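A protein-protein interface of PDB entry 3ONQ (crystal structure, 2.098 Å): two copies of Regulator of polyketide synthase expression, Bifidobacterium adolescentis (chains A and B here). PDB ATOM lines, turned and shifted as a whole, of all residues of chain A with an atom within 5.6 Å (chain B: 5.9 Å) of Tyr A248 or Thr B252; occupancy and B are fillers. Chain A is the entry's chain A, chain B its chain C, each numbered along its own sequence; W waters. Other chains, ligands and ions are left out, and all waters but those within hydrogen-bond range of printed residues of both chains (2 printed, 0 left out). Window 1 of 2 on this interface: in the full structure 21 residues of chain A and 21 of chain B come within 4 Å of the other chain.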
ATOM      1  N   PRO A 167     -25.817  33.677  23.382  1.00  0.00           N
ATOM      2  CA  PRO A 167     -25.693  32.239  23.637  1.00  0.00           C
ATOM      3  C   PRO A 167     -24.444  31.907  24.445  1.00  0.00           C
ATOM      4  O   PRO A 167     -24.505  31.055  25.324  1.00  0.00           O
ATOM      5  CB  PRO A 167     -25.597  31.633  22.230  1.00  0.00           C
ATOM      6  CG  PRO A 167     -26.241  32.619  21.342  1.00  0.00           C
ATOM      7  CD  PRO A 167     -25.880  33.977  21.941  1.00  0.00           C
ATOM      8  N   GLU A 168     -23.332  32.577  24.153  1.00  0.00           N
ATOM      9  CA  GLU A 168     -22.072  32.287  24.830  1.00  0.00           C
ATOM     10  C   GLU A 168     -22.126  32.634  26.320  1.00  0.00           C
ATOM     11  O   GLU A 168     -21.677  31.862  27.163  1.00  0.00           O
ATOM     12  CB  GLU A 168     -20.918  33.024  24.139  1.00  0.00           C
ATOM     13  CG  GLU A 168     -20.635  32.510  22.726  1.00  0.00           C
ATOM     14  CD  GLU A 168     -21.710  32.897  21.705  1.00  0.00           C
ATOM     15  OE1 GLU A 168     -22.425  33.909  21.912  1.00  0.00           O
ATOM     16  OE2 GLU A 168     -21.837  32.186  20.687  1.00  0.00           O
ATOM     17  N   LEU A 171     -24.161  30.045  27.915  1.00  0.00           N
ATOM     18  CA  LEU A 171     -23.348  28.840  28.108  1.00  0.00           C
ATOM     19  C   LEU A 171     -22.459  28.917  29.341  1.00  0.00           C
ATOM     20  O   LEU A 171     -22.189  27.898  29.965  1.00  0.00           O
ATOM     21  CB  LEU A 171     -22.484  28.571  26.876  1.00  0.00           C
ATOM     22  CG  LEU A 171     -23.276  28.058  25.668  1.00  0.00           C
ATOM     23  CD1 LEU A 171     -22.427  28.137  24.406  1.00  0.00           C
ATOM     24  CD2 LEU A 171     -23.777  26.629  25.927  1.00  0.00           C
ATOM     25  N   ASP A 243     -27.879  33.877   7.926  1.00  0.00           N
ATOM     26  CA  ASP A 243     -26.518  34.168   8.366  1.00  0.00           C
ATOM     27  C   ASP A 243     -26.156  33.146   9.425  1.00  0.00           C
ATOM     28  O   ASP A 243     -26.881  32.987  10.404  1.00  0.00           O
ATOM     29  CB  ASP A 243     -26.433  35.586   8.948  1.00  0.00           C
ATOM     30  CG  ASP A 243     -25.037  35.941   9.460  1.00  0.00           C
ATOM     31  OD1 ASP A 243     -24.549  37.041   9.151  1.00  0.00           O
ATOM     32  OD2 ASP A 243     -24.424  35.138  10.183  1.00  0.00           O
ATOM     33  N   PRO A 244     -25.033  32.443   9.234  1.00  0.00           N
ATOM     34  CA  PRO A 244     -24.636  31.390  10.184  1.00  0.00           C
ATOM     35  C   PRO A 244     -24.550  31.855  11.646  1.00  0.00           C
ATOM     36  O   PRO A 244     -24.972  31.122  12.539  1.00  0.00           O
ATOM     37  CB  PRO A 244     -23.268  30.947   9.659  1.00  0.00           C
ATOM     38  CG  PRO A 244     -23.334  31.231   8.177  1.00  0.00           C
ATOM     39  CD  PRO A 244     -24.139  32.510   8.058  1.00  0.00           C
ATOM     40  N   ARG A 245     -24.002  33.035  11.903  1.00  0.00           N
ATOM     41  CA  ARG A 245     -24.020  33.562  13.268  1.00  0.00           C
ATOM     42  C   ARG A 245     -25.452  33.711  13.799  1.00  0.00           C
ATOM     43  O   ARG A 245     -25.800  33.145  14.837  1.00  0.00           O
ATOM     44  CB  ARG A 245     -23.292  34.903  13.377  1.00  0.00           C
ATOM     45  CG  ARG A 245     -23.449  35.564  14.753  1.00  0.00           C
ATOM     46  CD  ARG A 245     -23.072  34.601  15.896  1.00  0.00           C
ATOM     47  NE  ARG A 245     -23.237  35.218  17.216  1.00  0.00           N
ATOM     48  CZ  ARG A 245     -23.119  34.561  18.369  1.00  0.00           C
ATOM     49  NH1 ARG A 245     -22.838  33.259  18.374  1.00  0.00           N
ATOM     50  NH2 ARG A 245     -23.283  35.201  19.523  1.00  0.00           N
ATOM     51  N   ASP A 246     -26.270  34.468  13.079  1.00  0.00           N
ATOM     52  CA  ASP A 246     -27.642  34.735  13.498  1.00  0.00           C
ATOM     53  C   ASP A 246     -28.432  33.442  13.695  1.00  0.00           C
ATOM     54  O   ASP A 246     -29.200  33.319  14.653  1.00  0.00           O
ATOM     55  CB  ASP A 246     -28.350  35.646  12.489  1.00  0.00           C
ATOM     56  CG  ASP A 246     -27.738  37.041  12.425  1.00  0.00           C
ATOM     57  OD1 ASP A 246     -26.587  37.225  12.877  1.00  0.00           O
ATOM     58  OD2 ASP A 246     -28.409  37.956  11.910  1.00  0.00           O
ATOM     59  N   ALA A 247     -28.227  32.478  12.796  1.00  0.00           N
ATOM     60  CA  ALA A 247     -28.877  31.178  12.894  1.00  0.00           C
ATOM     61  C   ALA A 247     -28.542  30.496  14.210  1.00  0.00           C
ATOM     62  O   ALA A 247     -29.399  29.856  14.809  1.00  0.00           O
ATOM     63  CB  ALA A 247     -28.505  30.261  11.687  1.00  0.00           C
ATOM     64  N   TYR A 248     -27.296  30.635  14.664  1.00  0.00           N
ATOM     65  CA  TYR A 248     -26.893  30.030  15.934  1.00  0.00           C
ATOM     66  C   TYR A 248     -27.600  30.718  17.115  1.00  0.00           C
ATOM     67  O   TYR A 248     -28.029  30.074  18.075  1.00  0.00           O
ATOM     68  CB  TYR A 248     -25.366  30.059  16.122  1.00  0.00           C
ATOM     69  CG  TYR A 248     -24.930  29.330  17.370  1.00  0.00           C
ATOM     70  CD1 TYR A 248     -24.863  27.942  17.398  1.00  0.00           C
ATOM     71  CD2 TYR A 248     -24.591  30.026  18.519  1.00  0.00           C
ATOM     72  CE1 TYR A 248     -24.476  27.272  18.545  1.00  0.00           C
ATOM     73  CE2 TYR A 248     -24.213  29.370  19.675  1.00  0.00           C
ATOM     74  CZ  TYR A 248     -24.160  27.994  19.683  1.00  0.00           C
ATOM     75  OH  TYR A 248     -23.791  27.337  20.829  1.00  0.00           O
ATOM     76  N   VAL A 249     -27.742  32.030  17.031  1.00  0.00           N
ATOM     77  CA  VAL A 249     -28.457  32.742  18.078  1.00  0.00           C
ATOM     78  C   VAL A 249     -29.925  32.280  18.126  1.00  0.00           C
ATOM     79  O   VAL A 249     -30.457  31.975  19.192  1.00  0.00           O
ATOM     80  CB  VAL A 249     -28.362  34.253  17.877  1.00  0.00           C
ATOM     81  CG1 VAL A 249     -29.186  34.978  18.941  1.00  0.00           C
ATOM     82  CG2 VAL A 249     -26.896  34.678  17.913  1.00  0.00           C
ATOM     83  N   LEU A 250     -30.563  32.211  16.963  1.00  0.00           N
ATOM     84  CA  LEU A 250     -31.961  31.791  16.872  1.00  0.00           C
ATOM     85  C   LEU A 250     -32.156  30.367  17.380  1.00  0.00           C
ATOM     86  O   LEU A 250     -33.111  30.080  18.111  1.00  0.00           O
ATOM     87  CB  LEU A 250     -32.457  31.903  15.425  1.00  0.00           C
ATOM     88  CG  LEU A 250     -32.690  33.347  14.950  1.00  0.00           C
ATOM     89  CD1 LEU A 250     -32.736  33.418  13.423  1.00  0.00           C
ATOM     90  CD2 LEU A 250     -33.960  33.934  15.569  1.00  0.00           C
ATOM     91  N   THR A 251     -31.241  29.473  17.010  1.00  0.00           N
ATOM     92  CA  THR A 251     -31.361  28.076  17.411  1.00  0.00           C
ATOM     93  C   THR A 251     -31.279  27.975  18.922  1.00  0.00           C
ATOM     94  O   THR A 251     -32.033  27.224  19.551  1.00  0.00           O
ATOM     95  CB  THR A 251     -30.262  27.196  16.765  1.00  0.00           C
ATOM     96  OG1 THR A 251     -30.449  27.156  15.348  1.00  0.00           O
ATOM     97  CG2 THR A 251     -30.339  25.798  17.301  1.00  0.00           C
ATOM     98  N   THR A 252     -30.358  28.742  19.501  1.00  0.00           N
ATOM     99  CA  THR A 252     -30.169  28.752  20.949  1.00  0.00           C
ATOM    100  C   THR A 252     -31.425  29.283  21.638  1.00  0.00           C
ATOM    101  O   THR A 252     -31.850  28.749  22.642  1.00  0.00           O
ATOM    102  CB  THR A 252     -28.990  29.654  21.346  1.00  0.00           C
ATOM    103  OG1 THR A 252     -27.828  29.226  20.640  1.00  0.00           O
ATOM    104  CG2 THR A 252     -28.724  29.596  22.870  1.00  0.00           C
ATOM    105  N   ALA A 253     -32.022  30.330  21.083  1.00  0.00           N
ATOM    106  CA  ALA A 253     -33.212  30.918  21.680  1.00  0.00           C
ATOM    107  C   ALA A 253     -34.359  29.910  21.657  1.00  0.00           C
ATOM    108  O   ALA A 253     -35.067  29.746  22.656  1.00  0.00           O
ATOM    109  CB  ALA A 253     -33.595  32.181  20.934  1.00  0.00           C
ATOM    110  N   LEU B 166     -25.774  17.478  24.616  1.00  0.00           N
ATOM    111  CA  LEU B 166     -24.688  18.271  25.206  1.00  0.00           C
ATOM    112  C   LEU B 166     -24.912  19.782  25.223  1.00  0.00           C
ATOM    113  O   LEU B 166     -24.789  20.407  26.273  1.00  0.00           O
ATOM    114  CB  LEU B 166     -23.354  17.998  24.493  1.00  0.00           C
ATOM    115  CG  LEU B 166     -22.603  16.768  24.954  1.00  0.00           C
ATOM    116  CD1 LEU B 166     -21.242  16.695  24.261  1.00  0.00           C
ATOM    117  CD2 LEU B 166     -22.462  16.783  26.483  1.00  0.00           C
ATOM    118  N   PRO B 167     -25.198  20.385  24.057  1.00  0.00           N
ATOM    119  CA  PRO B 167     -25.274  21.850  24.022  1.00  0.00           C
ATOM    120  C   PRO B 167     -26.399  22.377  24.897  1.00  0.00           C
ATOM    121  O   PRO B 167     -26.189  23.351  25.628  1.00  0.00           O
ATOM    122  CB  PRO B 167     -25.583  22.166  22.555  1.00  0.00           C
ATOM    123  CG  PRO B 167     -25.266  20.934  21.806  1.00  0.00           C
ATOM    124  CD  PRO B 167     -25.471  19.787  22.741  1.00  0.00           C
ATOM    125  N   ALA B 170     -25.474  22.103  28.499  1.00  0.00           N
ATOM    126  CA  ALA B 170     -24.567  23.207  28.834  1.00  0.00           C
ATOM    127  C   ALA B 170     -25.361  24.506  29.064  1.00  0.00           C
ATOM    128  O   ALA B 170     -25.103  25.245  30.023  1.00  0.00           O
ATOM    129  CB  ALA B 170     -23.510  23.391  27.737  1.00  0.00           C
ATOM    130  N   LEU B 181     -17.928  19.060  26.240  1.00  0.00           N
ATOM    131  CA  LEU B 181     -17.827  19.835  25.024  1.00  0.00           C
ATOM    132  C   LEU B 181     -16.385  20.279  24.836  1.00  0.00           C
ATOM    133  O   LEU B 181     -15.874  20.220  23.737  1.00  0.00           O
ATOM    134  CB  LEU B 181     -18.765  21.036  25.050  1.00  0.00           C
ATOM    135  CG  LEU B 181     -20.224  20.692  24.778  1.00  0.00           C
ATOM    136  CD1 LEU B 181     -21.152  21.756  25.268  1.00  0.00           C
ATOM    137  CD2 LEU B 181     -20.451  20.408  23.325  1.00  0.00           C
ATOM    138  N   ALA B 247     -23.685  19.836  13.502  1.00  0.00           N
ATOM    139  CA  ALA B 247     -23.039  21.114  13.240  1.00  0.00           C
ATOM    140  C   ALA B 247     -23.307  22.073  14.397  1.00  0.00           C
ATOM    141  O   ALA B 247     -22.429  22.820  14.819  1.00  0.00           O
ATOM    142  CB  ALA B 247     -23.533  21.711  11.924  1.00  0.00           C
ATOM    143  N   TYR B 248     -24.540  22.054  14.898  1.00  0.00           N
ATOM    144  CA  TYR B 248     -24.905  22.886  16.035  1.00  0.00           C
ATOM    145  C   TYR B 248     -24.090  22.487  17.279  1.00  0.00           C
ATOM    146  O   TYR B 248     -23.525  23.342  17.978  1.00  0.00           O
ATOM    147  CB  TYR B 248     -26.417  22.815  16.307  1.00  0.00           C
ATOM    148  CG  TYR B 248     -26.795  23.476  17.603  1.00  0.00           C
ATOM    149  CD1 TYR B 248     -26.718  24.855  17.754  1.00  0.00           C
ATOM    150  CD2 TYR B 248     -27.212  22.721  18.682  1.00  0.00           C
ATOM    151  CE1 TYR B 248     -27.049  25.458  18.953  1.00  0.00           C
ATOM    152  CE2 TYR B 248     -27.537  23.307  19.872  1.00  0.00           C
ATOM    153  CZ  TYR B 248     -27.455  24.666  20.009  1.00  0.00           C
ATOM    154  OH  TYR B 248     -27.792  25.223  21.215  1.00  0.00           O
ATOM    155  N   VAL B 249     -23.997  21.184  17.533  1.00  0.00           N
ATOM    156  CA  VAL B 249     -23.199  20.702  18.654  1.00  0.00           C
ATOM    157  C   VAL B 249     -21.744  21.164  18.523  1.00  0.00           C
ATOM    158  O   VAL B 249     -21.148  21.650  19.482  1.00  0.00           O
ATOM    159  CB  VAL B 249     -23.256  19.155  18.772  1.00  0.00           C
ATOM    160  CG1 VAL B 249     -22.359  18.673  19.878  1.00  0.00           C
ATOM    161  CG2 VAL B 249     -24.692  18.689  19.010  1.00  0.00           C
ATOM    162  N   LEU B 250     -21.179  21.022  17.329  1.00  0.00           N
ATOM    163  CA  LEU B 250     -19.781  21.388  17.091  1.00  0.00           C
ATOM    164  C   LEU B 250     -19.547  22.895  17.245  1.00  0.00           C
ATOM    165  O   LEU B 250     -18.524  23.322  17.802  1.00  0.00           O
ATOM    166  CB  LEU B 250     -19.329  20.912  15.703  1.00  0.00           C
ATOM    167  CG  LEU B 250     -19.090  19.406  15.590  1.00  0.00           C
ATOM    168  CD1 LEU B 250     -19.213  18.922  14.135  1.00  0.00           C
ATOM    169  CD2 LEU B 250     -17.723  19.045  16.178  1.00  0.00           C
ATOM    170  N   THR B 251     -20.490  23.693  16.749  1.00  0.00           N
ATOM    171  CA  THR B 251     -20.419  25.145  16.918  1.00  0.00           C
ATOM    172  C   THR B 251     -20.363  25.476  18.407  1.00  0.00           C
ATOM    173  O   THR B 251     -19.583  26.338  18.859  1.00  0.00           O
ATOM    174  CB  THR B 251     -21.637  25.853  16.278  1.00  0.00           C
ATOM    175  OG1 THR B 251     -21.676  25.567  14.873  1.00  0.00           O
ATOM    176  CG2 THR B 251     -21.544  27.350  16.475  1.00  0.00           C
ATOM    177  N   THR B 252     -21.180  24.777  19.176  1.00  0.00           N
ATOM    178  CA  THR B 252     -21.192  24.969  20.625  1.00  0.00           C
ATOM    179  C   THR B 252     -19.832  24.616  21.243  1.00  0.00           C
ATOM    180  O   THR B 252     -19.290  25.374  22.058  1.00  0.00           O
ATOM    181  CB  THR B 252     -22.338  24.165  21.286  1.00  0.00           C
ATOM    182  OG1 THR B 252     -23.591  24.572  20.716  1.00  0.00           O
ATOM    183  CG2 THR B 252     -22.384  24.412  22.804  1.00  0.00           C
ATOM    184  N   ALA B 253     -19.266  23.480  20.841  1.00  0.00           N
ATOM    185  CA  ALA B 253     -17.967  23.069  21.375  1.00  0.00           C
ATOM    186  C   ALA B 253     -16.875  24.097  21.048  1.00  0.00           C
ATOM    187  O   ALA B 253     -16.010  24.368  21.880  1.00  0.00           O
ATOM    188  CB  ALA B 253     -17.567  21.660  20.858  1.00  0.00           C
ATOM    189  N   LEU B 254     -16.910  24.679  19.847  1.00  0.00           N
ATOM    190  CA  LEU B 254     -15.917  25.701  19.499  1.00  0.00           C
ATOM    191  C   LEU B 254     -16.042  26.926  20.406  1.00  0.00           C
ATOM    192  O   LEU B 254     -15.044  27.477  20.867  1.00  0.00           O
ATOM    193  CB  LEU B 254     -15.999  26.115  18.020  1.00  0.00           C
ATOM    194  CG  LEU B 254     -15.733  25.020  16.973  1.00  0.00           C
ATOM    195  CD1 LEU B 254     -15.654  25.621  15.566  1.00  0.00           C
ATOM    196  CD2 LEU B 254     -14.478  24.257  17.257  1.00  0.00           C
ATOM    197  N   ALA B 255     -17.272  27.348  20.660  1.00  0.00           N
ATOM    198  CA  ALA B 255     -17.495  28.485  21.546  1.00  0.00           C
ATOM    199  C   ALA B 255     -16.968  28.155  22.953  1.00  0.00           C
ATOM    200  O   ALA B 255     -16.236  28.956  23.551  1.00  0.00           O
ATOM    201  CB  ALA B 255     -18.976  28.863  21.575  1.00  0.00           C
ATOM    202  N   ILE B 256     -17.305  26.971  23.465  1.00  0.00           N
ATOM    203  CA  ILE B 256     -16.838  26.565  24.798  1.00  0.00           C
ATOM    204  C   ILE B 256     -15.302  26.600  24.840  1.00  0.00           C
ATOM    205  O   ILE B 256     -14.691  27.163  25.756  1.00  0.00           O
ATOM    206  CB  ILE B 256     -17.329  25.146  25.182  1.00  0.00           C
ATOM    207  CG1 ILE B 256     -18.825  25.134  25.531  1.00  0.00           C
ATOM    208  CG2 ILE B 256     -16.490  24.573  26.340  1.00  0.00           C
ATOM    209  CD1 ILE B 256     -19.187  26.017  26.722  1.00  0.00           C
ATOM    210  N   GLY B 257     -14.682  26.010  23.825  1.00  0.00           N
ATOM    211  CA  GLY B 257     -13.237  25.923  23.767  1.00  0.00           C
ATOM    212  C   GLY B 257     -12.556  27.277  23.668  1.00  0.00           C
ATOM    213  O   GLY B 257     -11.565  27.532  24.347  1.00  0.00           O
HETATM  214  O   HOH W   1     -26.572  27.193  22.021  1.00  0.00           O
HETATM  215  O   HOH W   2     -25.140  27.556  31.373  1.00  0.00           O
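The side-chain hydroxyl (OH) of Tyr A248 sits at hydrogen-bond distance from the side-chain hydroxyl (OG1) of Thr B252 (2.8 Å).
The backbone carbonyl oxygen of Ala A247 sits at hydrogen-bond distance from the side-chain hydroxyl of Thr A251 (2.9 Å).
The backbone carbonyl oxygen (O) of Tyr B248 is in hydrogen-bond range of the side-chain hydroxyl (OG1) of Thr B252 (3.0 Å).
OG1 of Thr A252 lies within hydrogen-bond range of O of Tyr A248 (2.7 Å).
O of Ala B247 lies within hydrogen-bond range of OG1 of Thr B251, at 2.8 Å.
CB of Ala B170 touches CD2 of Leu A171 (3.7 Å).
CE1 of Tyr A248 touches CE1 of Tyr B248, at 3.2 Å.
Tyr A248 touches Thr B251 (CD1 to CG2, 3.5 Å).
CE1 of Tyr B248 touches CG2 of Thr A251, at 3.7 Å.
Glu A168 touches none of the printed residues of chain B.
Of the printed residues of chain B, Leu A171 touches Ala B170 (3.7 Å).
Of chain B, only Tyr B248 (3.2 Å), Thr B251 (3.5 Å) and Thr B252 (2.8 Å) come within 4 Å of Tyr A248.
Of the printed residues of chain A, Ala B170 touches Leu A171 (3.7 Å).
Of the printed residues of chain A, Tyr B248 touches Tyr A248 and Thr A251.
Leu B250 touches none of the printed residues of chain A.
Printed residues of chain A within 4 Å of Thr B251: Tyr A248 (3.5 Å).
Thr B252 touches one residue of chain A.
The nearest printed residue of chain A that does not touch Tyr B248 is Thr A252 (4.04 Å).
Of the 14 printed residues of chain A, 3 touch a printed residue of chain B.
Among the printed residues, no Asp or Glu carboxylate lies within 4 Å of a Lys or Arg side-chain nitrogen of the other chain.
Tyr A248 touches its own counterpart, Tyr B248.
Tyr A248 touches Thr B251, and with the chains exchanged Thr A251 touches Tyr B248.
Tyr A248 touches Thr B252, but with the chains exchanged Thr A252 does not touch Tyr B248 (4.04 Å).
Of the 5 pairs that touch across the chains among the printed residues, 3 have their exchanged pair printed and touching as well.
Water W1 lies within hydrogen-bond range of OH of Tyr B248 (2.5 Å), OG1 of Thr A252 (2.8 Å) and OH of Tyr A248 (3.0 Å).
Water W2 bridges the backbone carbonyl oxygen of Ala B170 (2.7 Å) and the backbone carbonyl oxygen of Leu A171 (3.3 Å).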
